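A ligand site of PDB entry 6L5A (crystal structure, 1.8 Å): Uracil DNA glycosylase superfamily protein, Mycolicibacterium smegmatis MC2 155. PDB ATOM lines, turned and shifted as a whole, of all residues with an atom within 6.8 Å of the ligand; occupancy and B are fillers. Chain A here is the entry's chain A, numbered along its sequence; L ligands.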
ATOM      1  N   GLY A   6     -12.819   4.925 -23.000  1.00  0.00           N
ATOM      2  CA  GLY A   6     -12.449   6.321 -23.024  1.00  0.00           C
ATOM      3  C   GLY A   6     -11.644   6.647 -24.270  1.00  0.00           C
ATOM      4  O   GLY A   6     -11.035   5.778 -24.892  1.00  0.00           O
ATOM      5  N   ALA A   7     -11.637   7.927 -24.629  1.00  0.00           N
ATOM      6  CA  ALA A   7     -11.014   8.313 -25.896  1.00  0.00           C
ATOM      7  C   ALA A   7      -9.493   8.315 -25.861  1.00  0.00           C
ATOM      8  O   ALA A   7      -8.872   8.349 -26.925  1.00  0.00           O
ATOM      9  CB  ALA A   7     -11.505   9.707 -26.317  1.00  0.00           C
ATOM     10  N   PHE A  10      -7.259   6.565 -28.284  1.00  0.00           N
ATOM     11  CA  PHE A  10      -7.577   6.890 -29.659  1.00  0.00           C
ATOM     12  C   PHE A  10      -7.062   8.248 -30.091  1.00  0.00           C
ATOM     13  O   PHE A  10      -7.161   8.587 -31.279  1.00  0.00           O
ATOM     14  CB  PHE A  10      -9.107   6.816 -29.872  1.00  0.00           C
ATOM     15  CG  PHE A  10      -9.684   5.454 -29.646  1.00  0.00           C
ATOM     16  CD1 PHE A  10      -9.668   4.498 -30.664  1.00  0.00           C
ATOM     17  CD2 PHE A  10     -10.202   5.103 -28.412  1.00  0.00           C
ATOM     18  CE1 PHE A  10     -10.193   3.220 -30.442  1.00  0.00           C
ATOM     19  CE2 PHE A  10     -10.723   3.838 -28.185  1.00  0.00           C
ATOM     20  CZ  PHE A  10     -10.712   2.894 -29.210  1.00  0.00           C
ATOM     21  N   ALA A  23      -9.012  11.579 -36.624  1.00  0.00           N
ATOM     22  CA  ALA A  23      -8.856  10.566 -35.589  1.00  0.00           C
ATOM     23  C   ALA A  23     -10.077  10.489 -34.693  1.00  0.00           C
ATOM     24  O   ALA A  23     -10.461   9.410 -34.228  1.00  0.00           O
ATOM     25  CB  ALA A  23      -7.598  10.862 -34.764  1.00  0.00           C
ATOM     26  N   ALA A  24     -10.713  11.637 -34.428  1.00  0.00           N
ATOM     27  CA  ALA A  24     -11.940  11.626 -33.651  1.00  0.00           C
ATOM     28  C   ALA A  24     -13.035  10.895 -34.399  1.00  0.00           C
ATOM     29  O   ALA A  24     -13.888  10.244 -33.762  1.00  0.00           O
ATOM     30  CB  ALA A  24     -12.399  13.058 -33.344  1.00  0.00           C
ATOM     31  N   GLY A  25     -13.041  10.986 -35.734  1.00  0.00           N
ATOM     32  CA  GLY A  25     -13.986  10.179 -36.497  1.00  0.00           C
ATOM     33  C   GLY A  25     -13.792   8.699 -36.266  1.00  0.00           C
ATOM     34  O   GLY A  25     -14.754   7.909 -36.322  1.00  0.00           O
ATOM     35  N   GLU A  26     -12.547   8.280 -36.009  1.00  0.00           N
ATOM     36  CA  GLU A  26     -12.261   6.867 -35.748  1.00  0.00           C
ATOM     37  C   GLU A  26     -12.362   6.477 -34.274  1.00  0.00           C
ATOM     38  O   GLU A  26     -12.152   5.307 -33.946  1.00  0.00           O
ATOM     39  CB  GLU A  26     -10.870   6.533 -36.292  1.00  0.00           C
ATOM     40  CG  GLU A  26     -10.754   6.772 -37.783  1.00  0.00           C
ATOM     41  CD  GLU A  26     -11.736   5.904 -38.557  1.00  0.00           C
ATOM     42  OE1 GLU A  26     -12.504   6.450 -39.375  1.00  0.00           O
ATOM     43  OE2 GLU A  26     -11.741   4.675 -38.331  1.00  0.00           O
ATOM     44  N   CYS A  27     -12.676   7.423 -33.387  1.00  0.00           N
ATOM     45  CA  CYS A  27     -12.680   7.170 -31.958  1.00  0.00           C
ATOM     46  C   CYS A  27     -13.772   6.178 -31.573  1.00  0.00           C
ATOM     47  O   CYS A  27     -14.915   6.297 -32.015  1.00  0.00           O
ATOM     48  CB  CYS A  27     -12.895   8.488 -31.182  1.00  0.00           C
ATOM     49  SG  CYS A  27     -12.899   8.298 -29.375  1.00  0.00           S
ATOM     50  N   ARG A  28     -13.422   5.191 -30.716  1.00  0.00           N
ATOM     51  CA  ARG A  28     -14.402   4.273 -30.155  1.00  0.00           C
ATOM     52  C   ARG A  28     -14.407   4.342 -28.624  1.00  0.00           C
ATOM     53  O   ARG A  28     -14.642   3.334 -27.947  1.00  0.00           O
ATOM     54  CB  ARG A  28     -14.156   2.845 -30.636  1.00  0.00           C
ATOM     55  CG  ARG A  28     -14.085   2.720 -32.171  1.00  0.00           C
ATOM     56  CD  ARG A  28     -15.351   3.253 -32.840  1.00  0.00           C
ATOM     57  NE  ARG A  28     -15.311   3.154 -34.296  1.00  0.00           N
ATOM     58  CZ  ARG A  28     -15.391   4.193 -35.139  1.00  0.00           C
ATOM     59  NH1 ARG A  28     -15.338   3.985 -36.452  1.00  0.00           N
ATOM     60  NH2 ARG A  28     -15.517   5.426 -34.685  1.00  0.00           N
ATOM     61  N   GLY A  29     -14.167   5.534 -28.079  1.00  0.00           N
ATOM     62  CA  GLY A  29     -14.034   5.720 -26.651  1.00  0.00           C
ATOM     63  C   GLY A  29     -15.334   5.650 -25.874  1.00  0.00           C
ATOM     64  O   GLY A  29     -15.311   5.510 -24.649  1.00  0.00           O
ATOM     65  N   CYS A  30     -16.463   5.763 -26.556  1.00  0.00           N
ATOM     66  CA  CYS A  30     -17.757   5.520 -25.932  1.00  0.00           C
ATOM     67  C   CYS A  30     -18.697   5.008 -27.016  1.00  0.00           C
ATOM     68  O   CYS A  30     -18.263   4.685 -28.126  1.00  0.00           O
ATOM     69  CB  CYS A  30     -18.282   6.775 -25.210  1.00  0.00           C
ATOM     70  SG  CYS A  30     -19.016   8.077 -26.247  1.00  0.00           S
ATOM     71  N   GLY A  31     -19.981   4.910 -26.696  1.00  0.00           N
ATOM     72  CA  GLY A  31     -20.874   4.319 -27.665  1.00  0.00           C
ATOM     73  C   GLY A  31     -21.425   5.259 -28.702  1.00  0.00           C
ATOM     74  O   GLY A  31     -22.042   4.800 -29.668  1.00  0.00           O
ATOM     75  N   LEU A  32     -21.166   6.561 -28.556  1.00  0.00           N
ATOM     76  CA  LEU A  32     -21.892   7.567 -29.329  1.00  0.00           C
ATOM     77  C   LEU A  32     -21.476   7.637 -30.793  1.00  0.00           C
ATOM     78  O   LEU A  32     -22.240   8.167 -31.614  1.00  0.00           O
ATOM     79  CB  LEU A  32     -21.733   8.927 -28.649  1.00  0.00           C
ATOM     80  CG  LEU A  32     -22.369   8.977 -27.253  1.00  0.00           C
ATOM     81  CD1 LEU A  32     -22.147  10.376 -26.620  1.00  0.00           C
ATOM     82  CD2 LEU A  32     -23.866   8.659 -27.290  1.00  0.00           C
ATOM     83  N   TYR A  33     -20.292   7.106 -31.153  1.00  0.00           N
ATOM     84  CA  TYR A  33     -19.880   7.085 -32.553  1.00  0.00           C
ATOM     85  C   TYR A  33     -20.876   6.331 -33.415  1.00  0.00           C
ATOM     86  O   TYR A  33     -20.973   6.594 -34.618  1.00  0.00           O
ATOM     87  CB  TYR A  33     -18.490   6.421 -32.721  1.00  0.00           C
ATOM     88  CG  TYR A  33     -18.631   4.934 -32.519  1.00  0.00           C
ATOM     89  CD1 TYR A  33     -18.811   4.058 -33.605  1.00  0.00           C
ATOM     90  CD2 TYR A  33     -18.690   4.404 -31.241  1.00  0.00           C
ATOM     91  CE1 TYR A  33     -19.020   2.697 -33.394  1.00  0.00           C
ATOM     92  CE2 TYR A  33     -18.894   3.056 -31.026  1.00  0.00           C
ATOM     93  CZ  TYR A  33     -19.073   2.214 -32.098  1.00  0.00           C
ATOM     94  OH  TYR A  33     -19.291   0.877 -31.855  1.00  0.00           O
ATOM     95  N   ARG A  34     -21.598   5.366 -32.841  1.00  0.00           N
ATOM     96  CA  ARG A  34     -22.296   4.380 -33.651  1.00  0.00           C
ATOM     97  C   ARG A  34     -23.420   5.012 -34.472  1.00  0.00           C
ATOM     98  O   ARG A  34     -23.487   4.818 -35.687  1.00  0.00           O
ATOM     99  CB  ARG A  34     -22.849   3.271 -32.764  1.00  0.00           C
ATOM    100  CG  ARG A  34     -23.209   2.028 -33.545  1.00  0.00           C
ATOM    101  CD  ARG A  34     -23.713   0.922 -32.624  1.00  0.00           C
ATOM    102  NE  ARG A  34     -24.602   1.447 -31.581  1.00  0.00           N
ATOM    103  CZ  ARG A  34     -25.919   1.522 -31.697  1.00  0.00           C
ATOM    104  NH1 ARG A  34     -26.512   1.109 -32.805  1.00  0.00           N
ATOM    105  NH2 ARG A  34     -26.653   2.013 -30.705  1.00  0.00           N
ATOM    106  N   ALA A  39     -18.065  12.553 -36.571  1.00  0.00           N
ATOM    107  CA  ALA A  39     -17.596  13.413 -35.500  1.00  0.00           C
ATOM    108  C   ALA A  39     -17.830  14.865 -35.888  1.00  0.00           C
ATOM    109  O   ALA A  39     -17.790  15.242 -37.065  1.00  0.00           O
ATOM    110  CB  ALA A  39     -16.104  13.194 -35.222  1.00  0.00           C
ATOM    111  N   ALA A  95     -17.797  19.610 -25.683  1.00  0.00           N
ATOM    112  CA  ALA A  95     -17.242  18.607 -24.771  1.00  0.00           C
ATOM    113  C   ALA A  95     -17.385  17.182 -25.321  1.00  0.00           C
ATOM    114  O   ALA A  95     -16.540  16.328 -25.040  1.00  0.00           O
ATOM    115  CB  ALA A  95     -17.921  18.717 -23.409  1.00  0.00           C
ATOM    116  N   VAL A  96     -18.442  16.901 -26.064  1.00  0.00           N
ATOM    117  CA  VAL A  96     -18.690  15.584 -26.629  1.00  0.00           C
ATOM    118  C   VAL A  96     -18.796  15.725 -28.142  1.00  0.00           C
ATOM    119  O   VAL A  96     -19.391  16.682 -28.634  1.00  0.00           O
ATOM    120  CB  VAL A  96     -19.963  14.946 -26.009  1.00  0.00           C
ATOM    121  CG1 VAL A  96     -20.425  13.746 -26.802  1.00  0.00           C
ATOM    122  CG2 VAL A  96     -19.666  14.548 -24.556  1.00  0.00           C
ATOM    123  N   LYS A  97     -18.164  14.815 -28.879  1.00  0.00           N
ATOM    124  CA  LYS A  97     -17.952  15.035 -30.302  1.00  0.00           C
ATOM    125  C   LYS A  97     -18.842  14.211 -31.217  1.00  0.00           C
ATOM    126  O   LYS A  97     -18.815  14.411 -32.442  1.00  0.00           O
ATOM    127  CB  LYS A  97     -16.469  14.853 -30.623  1.00  0.00           C
ATOM    128  CG  LYS A  97     -15.729  16.027 -29.897  1.00  0.00           C
ATOM    129  CD  LYS A  97     -14.281  16.236 -30.213  1.00  0.00           C
ATOM    130  CE  LYS A  97     -13.930  17.689 -29.935  1.00  0.00           C
ATOM    131  NZ  LYS A  97     -13.975  18.122 -28.475  1.00  0.00           N
ATOM    132  N   HIS A  98     -19.669  13.320 -30.673  1.00  0.00           N
ATOM    133  CA  HIS A  98     -20.661  12.594 -31.459  1.00  0.00           C
ATOM    134  C   HIS A  98     -22.049  12.867 -30.903  1.00  0.00           C
ATOM    135  O   HIS A  98     -22.262  12.773 -29.692  1.00  0.00           O
ATOM    136  CB  HIS A  98     -20.376  11.079 -31.463  1.00  0.00           C
ATOM    137  CG  HIS A  98     -19.278  10.670 -32.401  1.00  0.00           C
ATOM    138  ND1 HIS A  98     -18.048  10.250 -31.958  1.00  0.00           N
ATOM    139  CD2 HIS A  98     -19.249  10.557 -33.756  1.00  0.00           C
ATOM    140  CE1 HIS A  98     -17.288   9.918 -32.985  1.00  0.00           C
ATOM    141  NE2 HIS A  98     -17.996  10.088 -34.094  1.00  0.00           N
ATOM    142  N   PHE A  99     -22.979  13.192 -31.800  1.00  0.00           N
ATOM    143  CA  PHE A  99     -24.359  13.553 -31.468  1.00  0.00           C
ATOM    144  C   PHE A  99     -25.073  12.393 -30.793  1.00  0.00           C
ATOM    145  O   PHE A  99     -25.127  11.292 -31.322  1.00  0.00           O
ATOM    146  CB  PHE A  99     -25.069  13.923 -32.775  1.00  0.00           C
ATOM    147  CG  PHE A  99     -26.505  14.352 -32.632  1.00  0.00           C
ATOM    148  CD1 PHE A  99     -26.931  15.150 -31.578  1.00  0.00           C
ATOM    149  CD2 PHE A  99     -27.418  14.017 -33.633  1.00  0.00           C
ATOM    150  CE1 PHE A  99     -28.264  15.565 -31.508  1.00  0.00           C
ATOM    151  CE2 PHE A  99     -28.733  14.423 -33.559  1.00  0.00           C
ATOM    152  CZ  PHE A  99     -29.151  15.198 -32.491  1.00  0.00           C
ATOM    153  N   GLU A 119     -19.909   9.716 -20.396  1.00  0.00           N
ATOM    154  CA  GLU A 119     -19.600  10.039 -21.787  1.00  0.00           C
ATOM    155  C   GLU A 119     -18.754  11.311 -21.904  1.00  0.00           C
ATOM    156  O   GLU A 119     -17.842  11.390 -22.742  1.00  0.00           O
ATOM    157  CB  GLU A 119     -20.898  10.161 -22.588  1.00  0.00           C
ATOM    158  CG  GLU A 119     -21.502   8.786 -22.886  1.00  0.00           C
ATOM    159  CD  GLU A 119     -22.993   8.806 -23.257  1.00  0.00           C
ATOM    160  OE1 GLU A 119     -23.701   9.772 -22.909  1.00  0.00           O
ATOM    161  OE2 GLU A 119     -23.451   7.819 -23.861  1.00  0.00           O
ATOM    162  N   VAL A 121     -16.582  12.441 -19.673  1.00  0.00           N
ATOM    163  CA  VAL A 121     -15.210  12.137 -19.264  1.00  0.00           C
ATOM    164  C   VAL A 121     -14.529  11.294 -20.329  1.00  0.00           C
ATOM    165  O   VAL A 121     -13.333  11.454 -20.592  1.00  0.00           O
ATOM    166  CB  VAL A 121     -15.205  11.450 -17.896  1.00  0.00           C
ATOM    167  CG1 VAL A 121     -13.793  10.978 -17.552  1.00  0.00           C
ATOM    168  CG2 VAL A 121     -15.713  12.419 -16.836  1.00  0.00           C
ATOM    169  N   ALA A 122     -15.268  10.373 -20.958  1.00  0.00           N
ATOM    170  CA  ALA A 122     -14.702   9.569 -22.034  1.00  0.00           C
ATOM    171  C   ALA A 122     -14.185  10.445 -23.156  1.00  0.00           C
ATOM    172  O   ALA A 122     -13.150  10.133 -23.768  1.00  0.00           O
ATOM    173  CB  ALA A 122     -15.751   8.591 -22.570  1.00  0.00           C
ATOM    174  N   CYS A 123     -14.889  11.540 -23.461  1.00  0.00           N
ATOM    175  CA  CYS A 123     -14.525  12.368 -24.601  1.00  0.00           C
ATOM    176  C   CYS A 123     -13.534  13.479 -24.257  1.00  0.00           C
ATOM    177  O   CYS A 123     -12.949  14.084 -25.165  1.00  0.00           O
ATOM    178  CB  CYS A 123     -15.785  12.993 -25.219  1.00  0.00           C
ATOM    179  SG  CYS A 123     -15.651  13.340 -26.980  1.00  0.00           S
ATOM    180  N   ARG A 124     -13.362  13.769 -22.970  1.00  0.00           N
ATOM    181  CA  ARG A 124     -12.479  14.863 -22.546  1.00  0.00           C
ATOM    182  C   ARG A 124     -11.062  14.841 -23.156  1.00  0.00           C
ATOM    183  O   ARG A 124     -10.527  15.936 -23.434  1.00  0.00           O
ATOM    184  CB  ARG A 124     -12.419  14.852 -21.015  1.00  0.00           C
ATOM    185  CG  ARG A 124     -11.771  16.087 -20.394  1.00  0.00           C
ATOM    186  CD  ARG A 124     -11.591  15.887 -18.882  1.00  0.00           C
ATOM    187  NE  ARG A 124     -10.955  17.024 -18.215  1.00  0.00           N
ATOM    188  CZ  ARG A 124      -9.644  17.224 -18.109  1.00  0.00           C
ATOM    189  NH1 ARG A 124      -8.784  16.372 -18.662  1.00  0.00           N
ATOM    190  NH2 ARG A 124      -9.189  18.297 -17.473  1.00  0.00           N
ATOM    191  N   PRO A 125     -10.413  13.692 -23.385  1.00  0.00           N
ATOM    192  CA  PRO A 125      -9.078  13.749 -24.016  1.00  0.00           C
ATOM    193  C   PRO A 125      -9.041  14.506 -25.332  1.00  0.00           C
ATOM    194  O   PRO A 125      -7.982  15.049 -25.688  1.00  0.00           O
ATOM    195  CB  PRO A 125      -8.715  12.274 -24.206  1.00  0.00           C
ATOM    196  CG  PRO A 125      -9.420  11.575 -23.091  1.00  0.00           C
ATOM    197  CD  PRO A 125     -10.727  12.319 -22.924  1.00  0.00           C
ATOM    198  N   TRP A 126     -10.148  14.549 -26.089  1.00  0.00           N
ATOM    199  CA  TRP A 126     -10.128  15.369 -27.314  1.00  0.00           C
ATOM    200  C   TRP A 126     -10.018  16.852 -26.971  1.00  0.00           C
ATOM    201  O   TRP A 126      -9.292  17.591 -27.658  1.00  0.00           O
ATOM    202  CB  TRP A 126     -11.367  15.108 -28.194  1.00  0.00           C
ATOM    203  CG  TRP A 126     -11.339  13.721 -28.767  1.00  0.00           C
ATOM    204  CD1 TRP A 126     -12.172  12.687 -28.452  1.00  0.00           C
ATOM    205  CD2 TRP A 126     -10.405  13.216 -29.729  1.00  0.00           C
ATOM    206  NE1 TRP A 126     -11.814  11.565 -29.169  1.00  0.00           N
ATOM    207  CE2 TRP A 126     -10.727  11.858 -29.947  1.00  0.00           C
ATOM    208  CE3 TRP A 126      -9.325  13.780 -30.432  1.00  0.00           C
ATOM    209  CZ2 TRP A 126     -10.011  11.046 -30.833  1.00  0.00           C
ATOM    210  CZ3 TRP A 126      -8.610  12.962 -31.328  1.00  0.00           C
ATOM    211  CH2 TRP A 126      -8.954  11.621 -31.520  1.00  0.00           C
HETATM  212 FE1  LIG L   1     -16.110  11.342 -27.901  1.00  0.00          FE
HETATM  213 FE2  LIG L   1     -14.982   9.063 -28.890  1.00  0.00          FE
HETATM  214 FE3  LIG L   1     -17.245  10.035 -30.037  1.00  0.00          FE
HETATM  215 FE4  LIG L   1     -17.380   8.899 -27.542  1.00  0.00          FE
HETATM  216  S1  LIG L   1     -16.817   7.938 -29.451  1.00  0.00           S
HETATM  217  S2  LIG L   1     -18.245  10.833 -28.262  1.00  0.00           S
HETATM  218  S3  LIG L   1     -15.393   9.550 -26.800  1.00  0.00           S
HETATM  219  S4  LIG L   1     -15.262  11.017 -29.903  1.00  0.00           S
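N of Cys 30 lies close to S1 of the ligand (3.6 Å).
The backbone NH (N) of His 98 lies close to a sulfur (S2) of the ligand, at 3.7 Å.
The side-chain sulfur (SG) of Cys 27 binds an iron atom (FE2) of the ligand.
The indole nitrogen of Trp 126 sits close to a sulfur (S4) of the ligand, 3.6 Å away.
The side-chain sulfur (SG) of Cys 123 binds an iron atom (FE1) of the ligand (2.2 Å).
An iron atom (FE3) of the ligand is bound by a ring nitrogen (ND1) of His 98 (2.1 Å).
An iron atom (FE4) of the ligand is bound by the side-chain sulfur (SG) of Cys 30 (2.2 Å).
Ala 7 touches the ligand (CB to S3, 3.9 Å).
Gly 29 touches the ligand.
Leu 32 touches the ligand.
N of Tyr 33 touches S1 of the ligand, 3.96 Å away.
Val 96 touches the ligand.
Ala 122 touches the ligand (O to S3, 3.8 Å).
Hydrophobic or aromatic side chains that line the ligand: Ala 7, Leu 32, Tyr 33, Val 96, His 98 and Trp 126.
Within 4 Å of the ligand: Ala 7, Cys 27, Gly 29, Cys 30, Leu 32, Tyr 33, Val 96, His 98, Ala 122, Cys 123 and Trp 126.
The nearest printed residue that does not touch the ligand is Lys 97 (4.03 Å).
The backbone carbonyl oxygen (O) of Ala 95 lies close to the side-chain sulfur (SG) of Cys 123 (3.7 Å).
The backbone NH of Gly 29 lies close to the side-chain sulfur of Cys 27 (3.3 Å).
The side-chain sulfur (SG) of Cys 30 lies close to the backbone NH (N) of Leu 32.
N of Lys 97 sits close to SG of Cys 123, 3.5 Å away.
A ring nitrogen (NE2) of His 98 lies within hydrogen-bond range of the backbone NH of Ala 39, at 3.5 Å.
The indole nitrogen (NE1) of Trp 126 sits close to the side-chain sulfur (SG) of Cys 27 (3.4 Å).
The backbone carbonyl oxygen (O) of Ala 122 is in hydrogen-bond range of the backbone NH (N) of Ala 7 (2.8 Å).
O of Gly 29 sits at hydrogen-bond distance from N of Gly 6 (3.0 Å).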
